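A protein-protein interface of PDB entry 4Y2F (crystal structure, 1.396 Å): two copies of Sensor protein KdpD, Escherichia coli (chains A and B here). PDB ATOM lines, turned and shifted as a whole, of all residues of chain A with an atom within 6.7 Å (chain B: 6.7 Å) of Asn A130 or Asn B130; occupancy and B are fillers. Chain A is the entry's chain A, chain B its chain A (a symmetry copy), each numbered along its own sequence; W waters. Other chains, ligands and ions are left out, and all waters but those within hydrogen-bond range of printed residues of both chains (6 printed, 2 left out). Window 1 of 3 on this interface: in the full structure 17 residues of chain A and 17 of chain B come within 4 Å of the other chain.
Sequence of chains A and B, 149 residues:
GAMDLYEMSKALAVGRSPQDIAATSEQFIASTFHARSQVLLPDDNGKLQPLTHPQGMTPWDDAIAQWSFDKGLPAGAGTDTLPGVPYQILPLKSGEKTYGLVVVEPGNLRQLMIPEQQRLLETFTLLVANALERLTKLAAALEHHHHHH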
ATOM      1  N   SER A   9     -16.254 -35.969  11.256  1.00  0.00           N
ATOM      2  CA  SER A   9     -15.165 -35.008  11.075  1.00  0.00           C
ATOM      3  C   SER A   9     -14.668 -35.001   9.633  1.00  0.00           C
ATOM      4  O   SER A   9     -14.346 -33.938   9.082  1.00  0.00           O
ATOM      5  CB  SER A   9     -14.019 -35.291  12.056  1.00  0.00           C
ATOM      6  OG  SER A   9     -13.126 -36.274  11.553  1.00  0.00           O
ATOM      7  N   ALA A  13     -14.991 -31.682   7.293  1.00  0.00           N
ATOM      8  CA  ALA A  13     -13.761 -31.066   6.806  1.00  0.00           C
ATOM      9  C   ALA A  13     -13.913 -30.551   5.384  1.00  0.00           C
ATOM     10  O   ALA A  13     -13.229 -29.593   4.996  1.00  0.00           O
ATOM     11  CB  ALA A  13     -12.616 -32.074   6.865  1.00  0.00           C
ATOM     12  N   LEU A  92     -23.954 -24.413  19.765  1.00  0.00           N
ATOM     13  CA  LEU A  92     -22.767 -24.889  19.053  1.00  0.00           C
ATOM     14  C   LEU A  92     -21.643 -23.913  19.369  1.00  0.00           C
ATOM     15  O   LEU A  92     -21.492 -22.882  18.707  1.00  0.00           O
ATOM     16  CB  LEU A  92     -23.049 -24.951  17.559  1.00  0.00           C
ATOM     17  CG  LEU A  92     -24.279 -25.802  17.245  1.00  0.00           C
ATOM     18  CD1 LEU A  92     -24.665 -25.683  15.779  1.00  0.00           C
ATOM     19  CD2 LEU A  92     -24.044 -27.270  17.620  1.00  0.00           C
ATOM     20  N   LYS A  93     -20.842 -24.233  20.384  1.00  0.00           N
ATOM     21  CA  LYS A  93     -19.883 -23.293  20.933  1.00  0.00           C
ATOM     22  C   LYS A  93     -18.459 -23.750  20.674  1.00  0.00           C
ATOM     23  O   LYS A  93     -18.141 -24.938  20.792  1.00  0.00           O
ATOM     24  CB  LYS A  93     -20.036 -23.163  22.447  1.00  0.00           C
ATOM     25  CG  LYS A  93     -21.398 -22.766  22.915  1.00  0.00           C
ATOM     26  CD  LYS A  93     -21.421 -22.624  24.429  1.00  0.00           C
ATOM     27  CE  LYS A  93     -20.644 -21.410  24.892  1.00  0.00           C
ATOM     28  NZ  LYS A  93     -20.943 -21.085  26.328  1.00  0.00           N
ATOM     29  N   SER A  94     -17.605 -22.800  20.334  1.00  0.00           N
ATOM     30  CA  SER A  94     -16.168 -23.021  20.337  1.00  0.00           C
ATOM     31  C   SER A  94     -15.582 -21.971  21.264  1.00  0.00           C
ATOM     32  O   SER A  94     -15.675 -20.770  20.985  1.00  0.00           O
ATOM     33  CB  SER A  94     -15.588 -22.905  18.935  1.00  0.00           C
ATOM     34  OG  SER A  94     -14.185 -23.050  18.991  1.00  0.00           O
ATOM     35  N   GLY A  95     -15.003 -22.420  22.373  1.00  0.00           N
ATOM     36  CA  GLY A  95     -14.610 -21.477  23.402  1.00  0.00           C
ATOM     37  C   GLY A  95     -15.847 -20.837  24.000  1.00  0.00           C
ATOM     38  O   GLY A  95     -16.848 -21.508  24.284  1.00  0.00           O
ATOM     39  N   TYR A  99     -21.800 -20.233  17.687  1.00  0.00           N
ATOM     40  CA  TYR A  99     -21.891 -20.041  16.247  1.00  0.00           C
ATOM     41  C   TYR A  99     -23.216 -20.502  15.678  1.00  0.00           C
ATOM     42  O   TYR A  99     -23.481 -20.279  14.493  1.00  0.00           O
ATOM     43  CB  TYR A  99     -20.742 -20.784  15.550  1.00  0.00           C
ATOM     44  CG  TYR A  99     -19.412 -20.147  15.864  1.00  0.00           C
ATOM     45  CD1 TYR A  99     -18.703 -20.503  17.006  1.00  0.00           C
ATOM     46  CD2 TYR A  99     -18.895 -19.147  15.055  1.00  0.00           C
ATOM     47  CE1 TYR A  99     -17.512 -19.892  17.324  1.00  0.00           C
ATOM     48  CE2 TYR A  99     -17.699 -18.542  15.354  1.00  0.00           C
ATOM     49  CZ  TYR A  99     -17.011 -18.914  16.492  1.00  0.00           C
ATOM     50  OH  TYR A  99     -15.824 -18.296  16.798  1.00  0.00           O
ATOM     51  N   THR A 125     -21.216 -31.563  19.161  1.00  0.00           N
ATOM     52  CA  THR A 125     -21.490 -30.140  18.973  1.00  0.00           C
ATOM     53  C   THR A 125     -20.210 -29.315  18.935  1.00  0.00           C
ATOM     54  O   THR A 125     -20.164 -28.278  18.265  1.00  0.00           O
ATOM     55  CB  THR A 125     -22.444 -29.598  20.042  1.00  0.00           C
ATOM     56  OG1 THR A 125     -21.828 -29.645  21.337  1.00  0.00           O
ATOM     57  CG2 THR A 125     -23.755 -30.382  20.061  1.00  0.00           C
ATOM     58  N   LEU A 126     -19.157 -29.768  19.620  1.00  0.00           N
ATOM     59  CA  LEU A 126     -17.887 -29.058  19.560  1.00  0.00           C
ATOM     60  C   LEU A 126     -17.277 -29.150  18.166  1.00  0.00           C
ATOM     61  O   LEU A 126     -16.765 -28.154  17.638  1.00  0.00           O
ATOM     62  CB  LEU A 126     -16.939 -29.636  20.604  1.00  0.00           C
ATOM     63  CG  LEU A 126     -15.519 -29.099  20.666  1.00  0.00           C
ATOM     64  CD1 LEU A 126     -15.532 -27.576  20.815  1.00  0.00           C
ATOM     65  CD2 LEU A 126     -14.836 -29.740  21.845  1.00  0.00           C
ATOM     66  N   LEU A 127     -17.348 -30.325  17.541  1.00  0.00           N
ATOM     67  CA  LEU A 127     -16.815 -30.467  16.187  1.00  0.00           C
ATOM     68  C   LEU A 127     -17.635 -29.659  15.186  1.00  0.00           C
ATOM     69  O   LEU A 127     -17.072 -29.004  14.297  1.00  0.00           O
ATOM     70  CB  LEU A 127     -16.787 -31.942  15.797  1.00  0.00           C
ATOM     71  CG  LEU A 127     -15.788 -32.847  16.496  1.00  0.00           C
ATOM     72  CD1 LEU A 127     -15.722 -34.093  15.670  1.00  0.00           C
ATOM     73  CD2 LEU A 127     -14.413 -32.215  16.566  1.00  0.00           C
ATOM     74  N   VAL A 128     -18.965 -29.656  15.330  1.00  0.00           N
ATOM     75  CA  VAL A 128     -19.798 -28.831  14.464  1.00  0.00           C
ATOM     76  C   VAL A 128     -19.456 -27.355  14.635  1.00  0.00           C
ATOM     77  O   VAL A 128     -19.327 -26.609  13.654  1.00  0.00           O
ATOM     78  CB  VAL A 128     -21.288 -29.112  14.728  1.00  0.00           C
ATOM     79  CG1 VAL A 128     -22.142 -28.122  13.951  1.00  0.00           C
ATOM     80  CG2 VAL A 128     -21.617 -30.554  14.350  1.00  0.00           C
ATOM     81  N   ALA A 129     -19.297 -26.914  15.884  1.00  0.00           N
ATOM     82  CA  ALA A 129     -18.980 -25.518  16.148  1.00  0.00           C
ATOM     83  C   ALA A 129     -17.656 -25.120  15.513  1.00  0.00           C
ATOM     84  O   ALA A 129     -17.540 -24.027  14.957  1.00  0.00           O
ATOM     85  CB  ALA A 129     -18.945 -25.262  17.654  1.00  0.00           C
ATOM     86  N   ASN A 130     -16.649 -26.000  15.586  1.00  0.00           N
ATOM     87  CA  ASN A 130     -15.355 -25.716  14.969  1.00  0.00           C
ATOM     88  C   ASN A 130     -15.496 -25.535  13.464  1.00  0.00           C
ATOM     89  O   ASN A 130     -14.827 -24.682  12.870  1.00  0.00           O
ATOM     90  CB  ASN A 130     -14.383 -26.866  15.243  1.00  0.00           C
ATOM     91  CG  ASN A 130     -13.825 -26.854  16.645  1.00  0.00           C
ATOM     92  OD1 ASN A 130     -13.999 -25.893  17.390  1.00  0.00           O
ATOM     93  ND2 ASN A 130     -13.118 -27.920  17.004  1.00  0.00           N
ATOM     94  N   ALA A 131     -16.352 -26.337  12.827  1.00  0.00           N
ATOM     95  CA  ALA A 131     -16.553 -26.209  11.385  1.00  0.00           C
ATOM     96  C   ALA A 131     -17.229 -24.887  11.038  1.00  0.00           C
ATOM     97  O   ALA A 131     -16.805 -24.183  10.113  1.00  0.00           O
ATOM     98  CB  ALA A 131     -17.352 -27.404  10.861  1.00  0.00           C
ATOM     99  N   LEU A 132     -18.278 -24.532  11.782  1.00  0.00           N
ATOM    100  CA  LEU A 132     -18.939 -23.244  11.599  1.00  0.00           C
ATOM    101  C   LEU A 132     -17.981 -22.086  11.846  1.00  0.00           C
ATOM    102  O   LEU A 132     -17.986 -21.102  11.102  1.00  0.00           O
ATOM    103  CB  LEU A 132     -20.125 -23.150  12.554  1.00  0.00           C
ATOM    104  CG  LEU A 132     -21.279 -24.082  12.217  1.00  0.00           C
ATOM    105  CD1 LEU A 132     -22.381 -23.957  13.286  1.00  0.00           C
ATOM    106  CD2 LEU A 132     -21.825 -23.734  10.837  1.00  0.00           C
ATOM    107  N   GLU A 133     -17.140 -22.196  12.882  1.00  0.00           N
ATOM    108  CA  GLU A 133     -16.167 -21.141  13.166  1.00  0.00           C
ATOM    109  C   GLU A 133     -15.189 -20.971  12.012  1.00  0.00           C
ATOM    110  O   GLU A 133     -14.870 -19.845  11.613  1.00  0.00           O
ATOM    111  CB  GLU A 133     -15.425 -21.448  14.474  1.00  0.00           C
ATOM    112  CG  GLU A 133     -14.268 -20.492  14.812  1.00  0.00           C
ATOM    113  CD  GLU A 133     -13.527 -20.895  16.083  1.00  0.00           C
ATOM    114  OE1 GLU A 133     -13.579 -22.083  16.456  1.00  0.00           O
ATOM    115  OE2 GLU A 133     -12.889 -20.023  16.707  1.00  0.00           O
ATOM    116  N   ARG A 134     -14.715 -22.086  11.455  1.00  0.00           N
ATOM    117  CA  ARG A 134     -13.783 -22.018  10.341  1.00  0.00           C
ATOM    118  C   ARG A 134     -14.408 -21.316   9.140  1.00  0.00           C
ATOM    119  O   ARG A 134     -13.798 -20.420   8.545  1.00  0.00           O
ATOM    120  CB  ARG A 134     -13.307 -23.420   9.972  1.00  0.00           C
ATOM    121  CG  ARG A 134     -12.343 -23.414   8.808  1.00  0.00           C
ATOM    122  CD  ARG A 134     -11.827 -24.805   8.520  1.00  0.00           C
ATOM    123  NE  ARG A 134     -12.889 -25.691   8.051  1.00  0.00           N
ATOM    124  CZ  ARG A 134     -13.390 -26.703   8.753  1.00  0.00           C
ATOM    125  NH1 ARG A 134     -12.930 -26.968   9.973  1.00  0.00           N
ATOM    126  NH2 ARG A 134     -14.355 -27.451   8.232  1.00  0.00           N
ATOM    127  N   LEU A 135     -15.629 -21.708   8.769  1.00  0.00           N
ATOM    128  CA  LEU A 135     -16.257 -21.107   7.593  1.00  0.00           C
ATOM    129  C   LEU A 135     -16.568 -19.631   7.813  1.00  0.00           C
ATOM    130  O   LEU A 135     -16.354 -18.806   6.918  1.00  0.00           O
ATOM    131  CB  LEU A 135     -17.530 -21.864   7.219  1.00  0.00           C
ATOM    132  CG  LEU A 135     -17.377 -23.272   6.651  1.00  0.00           C
ATOM    133  CD1 LEU A 135     -18.738 -23.798   6.258  1.00  0.00           C
ATOM    134  CD2 LEU A 135     -16.436 -23.287   5.462  1.00  0.00           C
ATOM    135  N   SER B   9     -10.532 -27.298  24.530  1.00  0.00           N
ATOM    136  CA  SER B   9     -11.186 -26.586  23.431  1.00  0.00           C
ATOM    137  C   SER B   9     -11.293 -25.093  23.725  1.00  0.00           C
ATOM    138  O   SER B   9     -11.121 -24.258  22.824  1.00  0.00           O
ATOM    139  CB  SER B   9     -12.564 -27.193  23.131  1.00  0.00           C
ATOM    140  OG  SER B   9     -13.571 -26.652  23.973  1.00  0.00           O
ATOM    141  N   ALA B  13      -9.388 -22.333  21.413  1.00  0.00           N
ATOM    142  CA  ALA B  13     -10.206 -21.366  20.688  1.00  0.00           C
ATOM    143  C   ALA B  13      -9.561 -19.990  20.662  1.00  0.00           C
ATOM    144  O   ALA B  13      -9.795 -19.214  19.723  1.00  0.00           O
ATOM    145  CB  ALA B  13     -11.588 -21.271  21.328  1.00  0.00           C
ATOM    146  N   LEU B  92      -1.875 -35.178  13.208  1.00  0.00           N
ATOM    147  CA  LEU B  92      -2.944 -34.245  13.570  1.00  0.00           C
ATOM    148  C   LEU B  92      -3.745 -33.979  12.304  1.00  0.00           C
ATOM    149  O   LEU B  92      -3.399 -33.102  11.506  1.00  0.00           O
ATOM    150  CB  LEU B  92      -2.344 -32.964  14.131  1.00  0.00           C
ATOM    151  CG  LEU B  92      -1.407 -33.238  15.306  1.00  0.00           C
ATOM    152  CD1 LEU B  92      -0.663 -31.977  15.716  1.00  0.00           C
ATOM    153  CD2 LEU B  92      -2.175 -33.819  16.499  1.00  0.00           C
ATOM    154  N   LYS B  93      -4.825 -34.733  12.111  1.00  0.00           N
ATOM    155  CA  LYS B  93      -5.542 -34.743  10.850  1.00  0.00           C
ATOM    156  C   LYS B  93      -6.931 -34.151  11.005  1.00  0.00           C
ATOM    157  O   LYS B  93      -7.625 -34.409  11.994  1.00  0.00           O
ATOM    158  CB  LYS B  93      -5.725 -36.165  10.325  1.00  0.00           C
ATOM    159  CG  LYS B  93      -4.463 -36.944  10.149  1.00  0.00           C
ATOM    160  CD  LYS B  93      -4.762 -38.323   9.582  1.00  0.00           C
ATOM    161  CE  LYS B  93      -5.204 -38.253   8.136  1.00  0.00           C
ATOM    162  NZ  LYS B  93      -5.174 -39.609   7.489  1.00  0.00           N
ATOM    163  N   SER B  94      -7.334 -33.368  10.019  1.00  0.00           N
ATOM    164  CA  SER B  94      -8.724 -32.965   9.877  1.00  0.00           C
ATOM    165  C   SER B  94      -9.155 -33.419   8.493  1.00  0.00           C
ATOM    166  O   SER B  94      -8.623 -32.938   7.485  1.00  0.00           O
ATOM    167  CB  SER B  94      -8.881 -31.460  10.038  1.00  0.00           C
ATOM    168  OG  SER B  94     -10.229 -31.101   9.818  1.00  0.00           O
ATOM    169  N   GLY B  95     -10.094 -34.357   8.446  1.00  0.00           N
ATOM    170  CA  GLY B  95     -10.406 -34.988   7.179  1.00  0.00           C
ATOM    171  C   GLY B  95      -9.213 -35.797   6.711  1.00  0.00           C
ATOM    172  O   GLY B  95      -8.574 -36.516   7.489  1.00  0.00           O
ATOM    173  N   TYR B  99      -2.037 -31.700   9.424  1.00  0.00           N
ATOM    174  CA  TYR B  99      -1.546 -30.355   9.688  1.00  0.00           C
ATOM    175  C   TYR B  99      -0.337 -30.342  10.600  1.00  0.00           C
ATOM    176  O   TYR B  99       0.262 -29.282  10.803  1.00  0.00           O
ATOM    177  CB  TYR B  99      -2.667 -29.504  10.302  1.00  0.00           C
ATOM    178  CG  TYR B  99      -3.763 -29.243   9.301  1.00  0.00           C
ATOM    179  CD1 TYR B  99      -4.801 -30.152   9.127  1.00  0.00           C
ATOM    180  CD2 TYR B  99      -3.728 -28.122   8.486  1.00  0.00           C
ATOM    181  CE1 TYR B  99      -5.778 -29.943   8.182  1.00  0.00           C
ATOM    182  CE2 TYR B  99      -4.708 -27.896   7.551  1.00  0.00           C
ATOM    183  CZ  TYR B  99      -5.731 -28.810   7.398  1.00  0.00           C
ATOM    184  OH  TYR B  99      -6.699 -28.590   6.451  1.00  0.00           O
ATOM    185  N   THR B 125      -6.495 -35.254  19.343  1.00  0.00           N
ATOM    186  CA  THR B 125      -5.749 -34.869  18.146  1.00  0.00           C
ATOM    187  C   THR B 125      -6.656 -34.258  17.086  1.00  0.00           C
ATOM    188  O   THR B 125      -6.210 -33.405  16.310  1.00  0.00           O
ATOM    189  CB  THR B 125      -4.961 -36.045  17.563  1.00  0.00           C
ATOM    190  OG1 THR B 125      -5.853 -37.060  17.081  1.00  0.00           O
ATOM    191  CG2 THR B 125      -4.008 -36.639  18.599  1.00  0.00           C
ATOM    192  N   LEU B 126      -7.930 -34.656  17.052  1.00  0.00           N
ATOM    193  CA  LEU B 126      -8.859 -34.052  16.106  1.00  0.00           C
ATOM    194  C   LEU B 126      -9.112 -32.588  16.451  1.00  0.00           C
ATOM    195  O   LEU B 126      -9.141 -31.730  15.559  1.00  0.00           O
ATOM    196  CB  LEU B 126     -10.163 -34.840  16.109  1.00  0.00           C
ATOM    197  CG  LEU B 126     -11.312 -34.339  15.251  1.00  0.00           C
ATOM    198  CD1 LEU B 126     -10.857 -34.161  13.801  1.00  0.00           C
ATOM    199  CD2 LEU B 126     -12.425 -35.349  15.336  1.00  0.00           C
ATOM    200  N   LEU B 127      -9.266 -32.277  17.737  1.00  0.00           N
ATOM    201  CA  LEU B 127      -9.474 -30.886  18.135  1.00  0.00           C
ATOM    202  C   LEU B 127      -8.226 -30.049  17.876  1.00  0.00           C
ATOM    203  O   LEU B 127      -8.321 -28.911  17.393  1.00  0.00           O
ATOM    204  CB  LEU B 127      -9.869 -30.825  19.608  1.00  0.00           C
ATOM    205  CG  LEU B 127     -11.240 -31.348  20.001  1.00  0.00           C
ATOM    206  CD1 LEU B 127     -11.493 -30.824  21.379  1.00  0.00           C
ATOM    207  CD2 LEU B 127     -12.320 -30.847  19.065  1.00  0.00           C
ATOM    208  N   VAL B 128      -7.037 -30.600  18.152  1.00  0.00           N
ATOM    209  CA  VAL B 128      -5.805 -29.888  17.841  1.00  0.00           C
ATOM    210  C   VAL B 128      -5.695 -29.628  16.342  1.00  0.00           C
ATOM    211  O   VAL B 128      -5.343 -28.524  15.907  1.00  0.00           O
ATOM    212  CB  VAL B 128      -4.589 -30.660  18.383  1.00  0.00           C
ATOM    213  CG1 VAL B 128      -3.306 -30.002  17.899  1.00  0.00           C
ATOM    214  CG2 VAL B 128      -4.650 -30.716  19.907  1.00  0.00           C
ATOM    215  N   ALA B 129      -6.003 -30.643  15.532  1.00  0.00           N
ATOM    216  CA  ALA B 129      -5.918 -30.495  14.086  1.00  0.00           C
ATOM    217  C   ALA B 129      -6.856 -29.407  13.584  1.00  0.00           C
ATOM    218  O   ALA B 129      -6.485 -28.626  12.706  1.00  0.00           O
ATOM    219  CB  ALA B 129      -6.233 -31.825  13.402  1.00  0.00           C
ATOM    220  N   ASN B 130      -8.075 -29.342  14.135  1.00  0.00           N
ATOM    221  CA  ASN B 130      -9.025 -28.304  13.740  1.00  0.00           C
ATOM    222  C   ASN B 130      -8.476 -26.917  14.046  1.00  0.00           C
ATOM    223  O   ASN B 130      -8.679 -25.978  13.267  1.00  0.00           O
ATOM    224  CB  ASN B 130     -10.345 -28.493  14.491  1.00  0.00           C
ATOM    225  CG  ASN B 130     -11.192 -29.612  13.937  1.00  0.00           C
ATOM    226  OD1 ASN B 130     -10.909 -30.155  12.872  1.00  0.00           O
ATOM    227  ND2 ASN B 130     -12.263 -29.946  14.649  1.00  0.00           N
ATOM    228  N   ALA B 131      -7.789 -26.765  15.180  1.00  0.00           N
ATOM    229  CA  ALA B 131      -7.217 -25.466  15.529  1.00  0.00           C
ATOM    230  C   ALA B 131      -6.097 -25.081  14.570  1.00  0.00           C
ATOM    231  O   ALA B 131      -6.041 -23.944  14.085  1.00  0.00           O
ATOM    232  CB  ALA B 131      -6.733 -25.483  16.981  1.00  0.00           C
ATOM    233  N   LEU B 132      -5.201 -26.026  14.277  1.00  0.00           N
ATOM    234  CA  LEU B 132      -4.145 -25.794  13.297  1.00  0.00           C
ATOM    235  C   LEU B 132      -4.720 -25.479  11.922  1.00  0.00           C
ATOM    236  O   LEU B 132      -4.225 -24.585  11.229  1.00  0.00           O
ATOM    237  CB  LEU B 132      -3.256 -27.032  13.217  1.00  0.00           C
ATOM    238  CG  LEU B 132      -2.409 -27.279  14.456  1.00  0.00           C
ATOM    239  CD1 LEU B 132      -1.615 -28.589  14.294  1.00  0.00           C
ATOM    240  CD2 LEU B 132      -1.465 -26.101  14.668  1.00  0.00           C
ATOM    241  N   GLU B 133      -5.775 -26.196  11.519  1.00  0.00           N
ATOM    242  CA  GLU B 133      -6.405 -25.932  10.225  1.00  0.00           C
ATOM    243  C   GLU B 133      -6.972 -24.520  10.169  1.00  0.00           C
ATOM    244  O   GLU B 133      -6.814 -23.815   9.166  1.00  0.00           O
ATOM    245  CB  GLU B 133      -7.498 -26.973   9.950  1.00  0.00           C
ATOM    246  CG  GLU B 133      -8.341 -26.722   8.688  1.00  0.00           C
ATOM    247  CD  GLU B 133      -9.454 -27.750   8.512  1.00  0.00           C
ATOM    248  OE1 GLU B 133      -9.870 -28.360   9.515  1.00  0.00           O
ATOM    249  OE2 GLU B 133      -9.916 -27.944   7.369  1.00  0.00           O
ATOM    250  N   ARG B 134      -7.624 -24.089  11.249  1.00  0.00           N
ATOM    251  CA  ARG B 134      -8.189 -22.750  11.286  1.00  0.00           C
ATOM    252  C   ARG B 134      -7.105 -21.688  11.137  1.00  0.00           C
ATOM    253  O   ARG B 134      -7.240 -20.758  10.334  1.00  0.00           O
ATOM    254  CB  ARG B 134      -8.979 -22.553  12.578  1.00  0.00           C
ATOM    255  CG  ARG B 134      -9.581 -21.170  12.679  1.00  0.00           C
ATOM    256  CD  ARG B 134     -10.424 -21.032  13.926  1.00  0.00           C
ATOM    257  NE  ARG B 134      -9.614 -21.118  15.139  1.00  0.00           N
ATOM    258  CZ  ARG B 134      -9.642 -22.138  15.992  1.00  0.00           C
ATOM    259  NH1 ARG B 134     -10.442 -23.178  15.771  1.00  0.00           N
ATOM    260  NH2 ARG B 134      -8.866 -22.116  17.069  1.00  0.00           N
ATOM    261  N   LEU B 135      -6.018 -21.811  11.903  1.00  0.00           N
ATOM    262  CA  LEU B 135      -4.969 -20.794  11.840  1.00  0.00           C
ATOM    263  C   LEU B 135      -4.272 -20.786  10.484  1.00  0.00           C
ATOM    264  O   LEU B 135      -3.993 -19.717   9.930  1.00  0.00           O
ATOM    265  CB  LEU B 135      -3.949 -21.006  12.956  1.00  0.00           C
ATOM    266  CG  LEU B 135      -4.395 -20.728  14.389  1.00  0.00           C
ATOM    267  CD1 LEU B 135      -3.216 -20.903  15.318  1.00  0.00           C
ATOM    268  CD2 LEU B 135      -4.978 -19.334  14.522  1.00  0.00           C
HETATM  269  O   HOH W   1     -14.895 -29.751  12.760  1.00  0.00           O
HETATM  270  O   HOH W   2     -12.473 -24.726  20.111  1.00  0.00           O
HETATM  271  O   HOH W   3     -10.185 -26.960  18.008  1.00  0.00           O
HETATM  272  O   HOH W   4     -11.177 -25.697  11.940  1.00  0.00           O
HETATM  273  O   HOH W   5     -12.598 -31.950  10.630  1.00  0.00           O
HETATM  274  O   HOH W   6     -12.125 -24.181  13.599  1.00  0.00           O
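NH1 of Arg B134 lies within salt-bridge range of OE1 of Glu A133, at 3.4 Å. The guanidinium group of Arg A134 is in salt-bridge range of the side-chain carboxylate of Glu B133 (3.4 Å). The side-chain amide nitrogen (ND2) of Asn A130 lies close to the side-chain amide nitrogen (ND2) of Asn B130, at 3.2 Å.
The side-chain hydroxyl of Ser A94 lies within hydrogen-bond range of the side-chain amide oxygen of Asn A130 (3.3 Å). The side-chain carboxylate of Glu B133 is in hydrogen-bond range of the side-chain hydroxyl of Ser B94 (2.8 Å). OG of Ser B94 is in hydrogen-bond range of OD1 of Asn B130 (3.3 Å). The side-chain carboxylate (OE2) of Glu B133 sits close to the side-chain hydroxyl (OH) of Tyr B99. OG of Ser A94 lies within hydrogen-bond range of OE1 of Glu A133 (2.8 Å). The side-chain carboxylate (OE2) of Glu A133 lies close to the side-chain hydroxyl (OH) of Tyr A99, 3.4 Å away.
Among the printed residues, merely in contact across the chains: Ser A9 with Leu B126 (3.6 Å), Ala A13 with Ser B94 (3.9 Å), Ala A13 with Gly B95 (3.7 Å), Ser A94 with Ala B13 (3.9 Å), Gly A95 with Ala B13 (3.7 Å), Leu A126 with Ser B9 (3.6 Å), Leu A126 with Leu B127 (3.5 Å), Leu A127 with Leu B126 (3.5 Å), Leu A127 with Leu B127 (3.5 Å), Leu A127 with Asn B130 (3.7 Å) and Asn A130 with Leu B127 (3.7 Å).
Tyr A99 touches none of the printed residues of chain B. Of chain B, only Leu B127 and Asn B130 come within 4 Å of Asn A130. Ala A131 touches none of the printed residues of chain B. Printed residues of chain B within 4 Å of Glu A133: Arg B134. Printed residues of chain A within 4 Å of Leu B126: Ser A9 and Leu A127. Of chain A, only Leu A127 and Asn A130 come within 4 Å of Asn B130. Printed residues of chain A within 4 Å of Glu B133: Arg A134 (3.4 Å). The nearest residue of chain B that does not touch Asn A130 is Arg B134 (4.8 Å).
Of the 18 printed residues of chain A, 9 touch a printed residue of chain B. Hydrophobic or aromatic side chains of chain A within 4 Å of the printed part of chain B: Ala A13, Leu A126 and Leu A127. Along chain B the printed residues that touch a printed residue of chain A span positions 9 to 134.
Ser A9 touches Leu B126, and with the chains exchanged Leu A126 touches Ser B9. Ala A13 touches Gly B95, and with the chains exchanged Gly A95 touches Ala B13. Asn B130 touches its own counterpart, Asn A130. Glu A133 touches Arg B134, and with the chains exchanged Arg A134 touches Glu B133. Of the 14 pairs that touch across the chains among the printed residues, 14 have their exchanged pair printed and touching as well.
Water W5 lies within hydrogen-bond range of OG of Ser B94, O of Ser A9 and OD1 of Asn B130. Water W2 lies within hydrogen-bond range of the side-chain hydroxyl (OG) of Ser A94, the backbone carbonyl oxygen (O) of Ser B9 and the side-chain amide oxygen (OD1) of Asn A130. Water W1 lies within hydrogen-bond range of O of Leu A127 (2.8 Å) and ND2 of Asn B130 (3.2 Å). Water W3 bridges the backbone carbonyl oxygen of Leu B127 and the side-chain amide nitrogen of Asn A130. Water W6 lies within hydrogen-bond range of O of Asn A130 (2.8 Å) and NH1 of Arg B134 (2.9 Å). Water W4 lies within hydrogen-bond range of O of Asn B130 (2.8 Å) and NH1 of Arg A134 (2.9 Å).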
